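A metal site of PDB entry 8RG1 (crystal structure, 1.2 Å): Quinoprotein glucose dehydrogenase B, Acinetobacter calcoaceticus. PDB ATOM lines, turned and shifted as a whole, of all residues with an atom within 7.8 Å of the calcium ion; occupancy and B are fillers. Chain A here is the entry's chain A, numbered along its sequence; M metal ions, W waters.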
ATOM      1  N   SER A 250     -24.126  12.183  15.784  1.00  0.00           N
ATOM      2  CA  SER A 250     -23.478  13.280  15.104  1.00  0.00           C
ATOM      3  C   SER A 250     -22.035  12.868  14.895  1.00  0.00           C
ATOM      4  O   SER A 250     -21.583  11.847  15.414  1.00  0.00           O
ATOM      5  CB  SER A 250     -23.488  14.542  15.955  1.00  0.00           C
ATOM      6  OG  SER A 250     -22.772  14.301  17.149  1.00  0.00           O
ATOM      7  N   ASP A 251     -21.312  13.689  14.140  1.00  0.00           N
ATOM      8  CA  ASP A 251     -19.874  13.683  14.164  1.00  0.00           C
ATOM      9  C   ASP A 251     -19.293  12.354  13.684  1.00  0.00           C
ATOM     10  O   ASP A 251     -18.350  11.831  14.264  1.00  0.00           O
ATOM     11  CB  ASP A 251     -19.358  14.032  15.559  1.00  0.00           C
ATOM     12  CG  ASP A 251     -19.646  15.474  15.931  1.00  0.00           C
ATOM     13  OD1 ASP A 251     -19.001  16.354  15.364  1.00  0.00           O
ATOM     14  OD2 ASP A 251     -20.543  15.727  16.770  1.00  0.00           O
ATOM     15  N   GLU A 253     -16.648  10.952  11.236  1.00  0.00           N
ATOM     16  CA  GLU A 253     -15.367  11.609  11.076  1.00  0.00           C
ATOM     17  C   GLU A 253     -14.603  11.068   9.890  1.00  0.00           C
ATOM     18  O   GLU A 253     -14.652   9.893   9.592  1.00  0.00           O
ATOM     19  CB  GLU A 253     -14.458  11.421  12.284  1.00  0.00           C
ATOM     20  CG  GLU A 253     -15.030  12.016  13.525  1.00  0.00           C
ATOM     21  CD  GLU A 253     -14.188  11.772  14.755  1.00  0.00           C
ATOM     22  OE1 GLU A 253     -13.314  10.902  14.740  1.00  0.00           O
ATOM     23  OE2 GLU A 253     -14.411  12.448  15.756  1.00  0.00           O
ATOM     24  N   ASN A 267     -14.992  10.393  24.953  1.00  0.00           N
ATOM     25  CA  ASN A 267     -15.076  11.669  25.606  1.00  0.00           C
ATOM     26  C   ASN A 267     -15.332  12.808  24.645  1.00  0.00           C
ATOM     27  O   ASN A 267     -15.918  13.817  25.047  1.00  0.00           O
ATOM     28  CB  ASN A 267     -13.791  11.915  26.373  1.00  0.00           C
ATOM     29  CG  ASN A 267     -13.637  10.974  27.494  1.00  0.00           C
ATOM     30  OD1 ASN A 267     -14.081  11.248  28.630  1.00  0.00           O
ATOM     31  ND2 ASN A 267     -13.123   9.815  27.181  1.00  0.00           N
ATOM     32  N   VAL A 268     -14.917  12.666  23.385  1.00  0.00           N
ATOM     33  CA  VAL A 268     -15.050  13.710  22.389  1.00  0.00           C
ATOM     34  C   VAL A 268     -15.549  13.069  21.112  1.00  0.00           C
ATOM     35  O   VAL A 268     -14.925  12.132  20.632  1.00  0.00           O
ATOM     36  CB  VAL A 268     -13.729  14.417  22.102  1.00  0.00           C
ATOM     37  CG1 VAL A 268     -13.943  15.534  21.118  1.00  0.00           C
ATOM     38  CG2 VAL A 268     -13.119  14.937  23.380  1.00  0.00           C
ATOM     39  N   ALA A 269     -16.684  13.548  20.606  1.00  0.00           N
ATOM     40  CA  ALA A 269     -17.199  13.211  19.289  1.00  0.00           C
ATOM     41  C   ALA A 269     -16.829  14.344  18.340  1.00  0.00           C
ATOM     42  O   ALA A 269     -17.234  15.475  18.556  1.00  0.00           O
ATOM     43  CB  ALA A 269     -18.711  13.056  19.319  1.00  0.00           C
ATOM     44  N   GLY A 270     -16.087  14.030  17.291  1.00  0.00           N
ATOM     45  CA  GLY A 270     -15.755  15.093  16.367  1.00  0.00           C
ATOM     46  C   GLY A 270     -14.741  16.042  16.966  1.00  0.00           C
ATOM     47  O   GLY A 270     -13.758  15.634  17.599  1.00  0.00           O
ATOM     48  N   TYR A 271     -14.959  17.323  16.752  1.00  0.00           N
ATOM     49  CA  TYR A 271     -14.092  18.320  17.343  1.00  0.00           C
ATOM     50  C   TYR A 271     -14.342  18.399  18.846  1.00  0.00           C
ATOM     51  O   TYR A 271     -15.423  18.073  19.348  1.00  0.00           O
ATOM     52  CB  TYR A 271     -14.369  19.675  16.726  1.00  0.00           C
ATOM     53  CG  TYR A 271     -14.193  19.687  15.240  1.00  0.00           C
ATOM     54  CD1 TYR A 271     -12.928  19.705  14.671  1.00  0.00           C
ATOM     55  CD2 TYR A 271     -15.278  19.600  14.412  1.00  0.00           C
ATOM     56  CE1 TYR A 271     -12.769  19.681  13.302  1.00  0.00           C
ATOM     57  CE2 TYR A 271     -15.135  19.594  13.041  1.00  0.00           C
ATOM     58  CZ  TYR A 271     -13.879  19.633  12.490  1.00  0.00           C
ATOM     59  OH  TYR A 271     -13.721  19.628  11.138  1.00  0.00           O
ATOM     60  N   LYS A 272     -13.351  18.908  19.554  1.00  0.00           N
ATOM     61  CA  LYS A 272     -13.541  19.198  20.968  1.00  0.00           C
ATOM     62  C   LYS A 272     -14.197  20.567  21.069  1.00  0.00           C
ATOM     63  O   LYS A 272     -13.549  21.597  21.277  1.00  0.00           O
ATOM     64  CB  LYS A 272     -12.232  19.105  21.720  1.00  0.00           C
ATOM     65  CG  LYS A 272     -12.438  19.175  23.194  1.00  0.00           C
ATOM     66  CD  LYS A 272     -11.176  19.403  23.937  1.00  0.00           C
ATOM     67  CE  LYS A 272     -10.252  18.210  23.856  1.00  0.00           C
ATOM     68  NZ  LYS A 272      -9.113  18.394  24.781  1.00  0.00           N
ATOM     69  N   ASP A 273     -15.516  20.576  20.904  1.00  0.00           N
ATOM     70  CA  ASP A 273     -16.264  21.802  20.719  1.00  0.00           C
ATOM     71  C   ASP A 273     -17.441  21.949  21.666  1.00  0.00           C
ATOM     72  O   ASP A 273     -18.084  22.995  21.633  1.00  0.00           O
ATOM     73  CB  ASP A 273     -16.737  21.950  19.264  1.00  0.00           C
ATOM     74  CG  ASP A 273     -17.520  20.735  18.741  1.00  0.00           C
ATOM     75  OD1 ASP A 273     -17.941  19.868  19.558  1.00  0.00           O
ATOM     76  OD2 ASP A 273     -17.757  20.720  17.511  1.00  0.00           O
ATOM     77  N   ASP A 274     -17.750  20.942  22.468  1.00  0.00           N
ATOM     78  CA  ASP A 274     -18.907  20.964  23.352  1.00  0.00           C
ATOM     79  C   ASP A 274     -20.176  21.288  22.582  1.00  0.00           C
ATOM     80  O   ASP A 274     -21.046  22.016  23.049  1.00  0.00           O
ATOM     81  CB  ASP A 274     -18.732  21.953  24.505  1.00  0.00           C
ATOM     82  CG  ASP A 274     -17.706  21.538  25.520  1.00  0.00           C
ATOM     83  OD1 ASP A 274     -17.148  20.443  25.444  1.00  0.00           O
ATOM     84  OD2 ASP A 274     -17.457  22.377  26.416  1.00  0.00           O
ATOM     85  N   SER A 275     -20.269  20.796  21.353  1.00  0.00           N
ATOM     86  CA  SER A 275     -21.349  21.188  20.464  1.00  0.00           C
ATOM     87  C   SER A 275     -22.076  19.953  19.980  1.00  0.00           C
ATOM     88  O   SER A 275     -21.562  19.234  19.129  1.00  0.00           O
ATOM     89  CB  SER A 275     -20.795  21.969  19.275  1.00  0.00           C
ATOM     90  OG  SER A 275     -21.842  22.503  18.511  1.00  0.00           O
ATOM     91  N   GLY A 276     -23.286  19.735  20.511  1.00  0.00           N
ATOM     92  CA  GLY A 276     -24.158  18.693  20.012  1.00  0.00           C
ATOM     93  C   GLY A 276     -23.901  17.302  20.546  1.00  0.00           C
ATOM     94  O   GLY A 276     -24.644  16.381  20.195  1.00  0.00           O
ATOM     95  N   TYR A 277     -22.911  17.137  21.423  1.00  0.00           N
ATOM     96  CA  TYR A 277     -22.579  15.866  22.017  1.00  0.00           C
ATOM     97  C   TYR A 277     -21.992  16.130  23.375  1.00  0.00           C
ATOM     98  O   TYR A 277     -21.266  17.111  23.568  1.00  0.00           O
ATOM     99  CB  TYR A 277     -21.554  15.103  21.202  1.00  0.00           C
ATOM    100  CG  TYR A 277     -21.044  13.850  21.885  1.00  0.00           C
ATOM    101  CD1 TYR A 277     -21.749  12.668  21.837  1.00  0.00           C
ATOM    102  CD2 TYR A 277     -19.824  13.851  22.583  1.00  0.00           C
ATOM    103  CE1 TYR A 277     -21.276  11.548  22.450  1.00  0.00           C
ATOM    104  CE2 TYR A 277     -19.349  12.710  23.189  1.00  0.00           C
ATOM    105  CZ  TYR A 277     -20.098  11.555  23.145  1.00  0.00           C
ATOM    106  OH  TYR A 277     -19.656  10.384  23.745  1.00  0.00           O
ATOM    107  N   ALA A 278     -22.293  15.269  24.327  1.00  0.00           N
ATOM    108  CA  ALA A 278     -21.563  15.197  25.572  1.00  0.00           C
ATOM    109  C   ALA A 278     -21.456  13.730  25.944  1.00  0.00           C
ATOM    110  O   ALA A 278     -22.228  12.911  25.459  1.00  0.00           O
ATOM    111  CB  ALA A 278     -22.211  15.976  26.691  1.00  0.00           C
ATOM    112  N   ASN A 296     -27.765  12.201  22.286  1.00  0.00           N
ATOM    113  CA  ASN A 296     -26.354  12.429  22.091  1.00  0.00           C
ATOM    114  C   ASN A 296     -25.668  12.987  23.318  1.00  0.00           C
ATOM    115  O   ASN A 296     -24.620  13.624  23.203  1.00  0.00           O
ATOM    116  CB  ASN A 296     -26.087  13.307  20.875  1.00  0.00           C
ATOM    117  CG  ASN A 296     -24.997  12.775  20.009  1.00  0.00           C
ATOM    118  OD1 ASN A 296     -24.810  11.556  19.909  1.00  0.00           O
ATOM    119  ND2 ASN A 296     -24.299  13.664  19.331  1.00  0.00           N
ATOM    120  N   GLU A 309     -17.089  17.633  26.498  1.00  0.00           N
ATOM    121  CA  GLU A 309     -15.875  17.367  25.741  1.00  0.00           C
ATOM    122  C   GLU A 309     -14.708  18.157  26.293  1.00  0.00           C
ATOM    123  O   GLU A 309     -13.592  17.649  26.391  1.00  0.00           O
ATOM    124  CB  GLU A 309     -16.104  17.694  24.290  1.00  0.00           C
ATOM    125  CG  GLU A 309     -17.175  16.833  23.693  1.00  0.00           C
ATOM    126  CD  GLU A 309     -17.331  17.070  22.225  1.00  0.00           C
ATOM    127  OE1 GLU A 309     -17.206  18.225  21.810  1.00  0.00           O
ATOM    128  OE2 GLU A 309     -17.538  16.087  21.479  1.00  0.00           O
ATOM    129  N   PHE A 317      -4.802  14.271  21.868  1.00  0.00           N
ATOM    130  CA  PHE A 317      -6.082  14.331  21.196  1.00  0.00           C
ATOM    131  C   PHE A 317      -5.910  14.919  19.796  1.00  0.00           C
ATOM    132  O   PHE A 317      -5.390  16.019  19.630  1.00  0.00           O
ATOM    133  CB  PHE A 317      -7.103  15.172  21.961  1.00  0.00           C
ATOM    134  CG  PHE A 317      -8.339  15.393  21.155  1.00  0.00           C
ATOM    135  CD1 PHE A 317      -9.115  14.309  20.756  1.00  0.00           C
ATOM    136  CD2 PHE A 317      -8.699  16.635  20.713  1.00  0.00           C
ATOM    137  CE1 PHE A 317     -10.229  14.485  19.984  1.00  0.00           C
ATOM    138  CE2 PHE A 317      -9.824  16.817  19.933  1.00  0.00           C
ATOM    139  CZ  PHE A 317     -10.566  15.726  19.550  1.00  0.00           C
ATOM    140  N   PRO A 320     -10.739  15.482  14.048  1.00  0.00           N
ATOM    141  CA  PRO A 320     -10.958  14.995  12.688  1.00  0.00           C
ATOM    142  C   PRO A 320     -10.615  16.040  11.652  1.00  0.00           C
ATOM    143  O   PRO A 320     -10.669  17.236  11.896  1.00  0.00           O
ATOM    144  CB  PRO A 320     -12.448  14.713  12.665  1.00  0.00           C
ATOM    145  CG  PRO A 320     -13.005  15.653  13.665  1.00  0.00           C
ATOM    146  CD  PRO A 320     -11.998  15.712  14.757  1.00  0.00           C
ATOM    147  N   THR A 323     -15.978  16.465   9.836  1.00  0.00           N
ATOM    148  CA  THR A 323     -17.091  15.799  10.499  1.00  0.00           C
ATOM    149  C   THR A 323     -18.291  15.796   9.565  1.00  0.00           C
ATOM    150  O   THR A 323     -18.592  16.786   8.900  1.00  0.00           O
ATOM    151  CB  THR A 323     -17.481  16.471  11.805  1.00  0.00           C
ATOM    152  OG1 THR A 323     -17.772  17.843  11.523  1.00  0.00           O
ATOM    153  CG2 THR A 323     -16.391  16.270  12.837  1.00  0.00           C
ATOM    154  N   THR A 326     -21.430  18.099  12.222  1.00  0.00           N
ATOM    155  CA  THR A 326     -21.454  18.740  13.524  1.00  0.00           C
ATOM    156  C   THR A 326     -22.632  19.690  13.603  1.00  0.00           C
ATOM    157  O   THR A 326     -22.914  20.415  12.653  1.00  0.00           O
ATOM    158  CB  THR A 326     -20.157  19.480  13.778  1.00  0.00           C
ATOM    159  OG1 THR A 326     -19.092  18.534  13.725  1.00  0.00           O
ATOM    160  CG2 THR A 326     -20.186  20.127  15.146  1.00  0.00           C
ATOM    161  N   VAL A 327     -23.320  19.651  14.735  1.00  0.00           N
ATOM    162  CA  VAL A 327     -24.472  20.490  14.988  1.00  0.00           C
ATOM    163  C   VAL A 327     -24.284  21.142  16.351  1.00  0.00           C
ATOM    164  O   VAL A 327     -23.402  20.778  17.137  1.00  0.00           O
ATOM    165  CB  VAL A 327     -25.778  19.679  14.934  1.00  0.00           C
ATOM    166  CG1 VAL A 327     -25.942  19.111  13.552  1.00  0.00           C
ATOM    167  CG2 VAL A 327     -25.817  18.585  16.000  1.00  0.00           C
HETATM  168 CA    CA M   1     -17.658  17.523  19.474  1.00  0.00          CA
HETATM  169  O   HOH W   1     -19.913  17.085  19.078  1.00  0.00           O
HETATM  170  O   HOH W   2     -17.733  18.091  17.043  1.00  0.00           O
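The calcium ion is bound by O of Ala 269, O of Tyr 271, water W1, OD1 of Asp 273, OE2 of Glu 309, OE1 of Glu 309 and water W2.
The calcium ion has seven donor atoms within binding distance.
Water W2 lies within hydrogen-bond range of OD2 of Asp 273 (2.7 Å), OD1 of Asp 251 (2.7 Å) and N of Tyr 271 (2.9 Å).
Water W1 lies within hydrogen-bond range of the backbone carbonyl oxygen (O) of Ser 275 (2.7 Å) and the side-chain carboxylate (OD2) of Asp 251 (2.8 Å).
The side-chain carboxylate (OD1) of Asp 273 lies close to the backbone NH (N) of Ser 275, 3.1 Å away.
N of Glu 309 sits at hydrogen-bond distance from OD1 of Asp 274 (3.0 Å).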
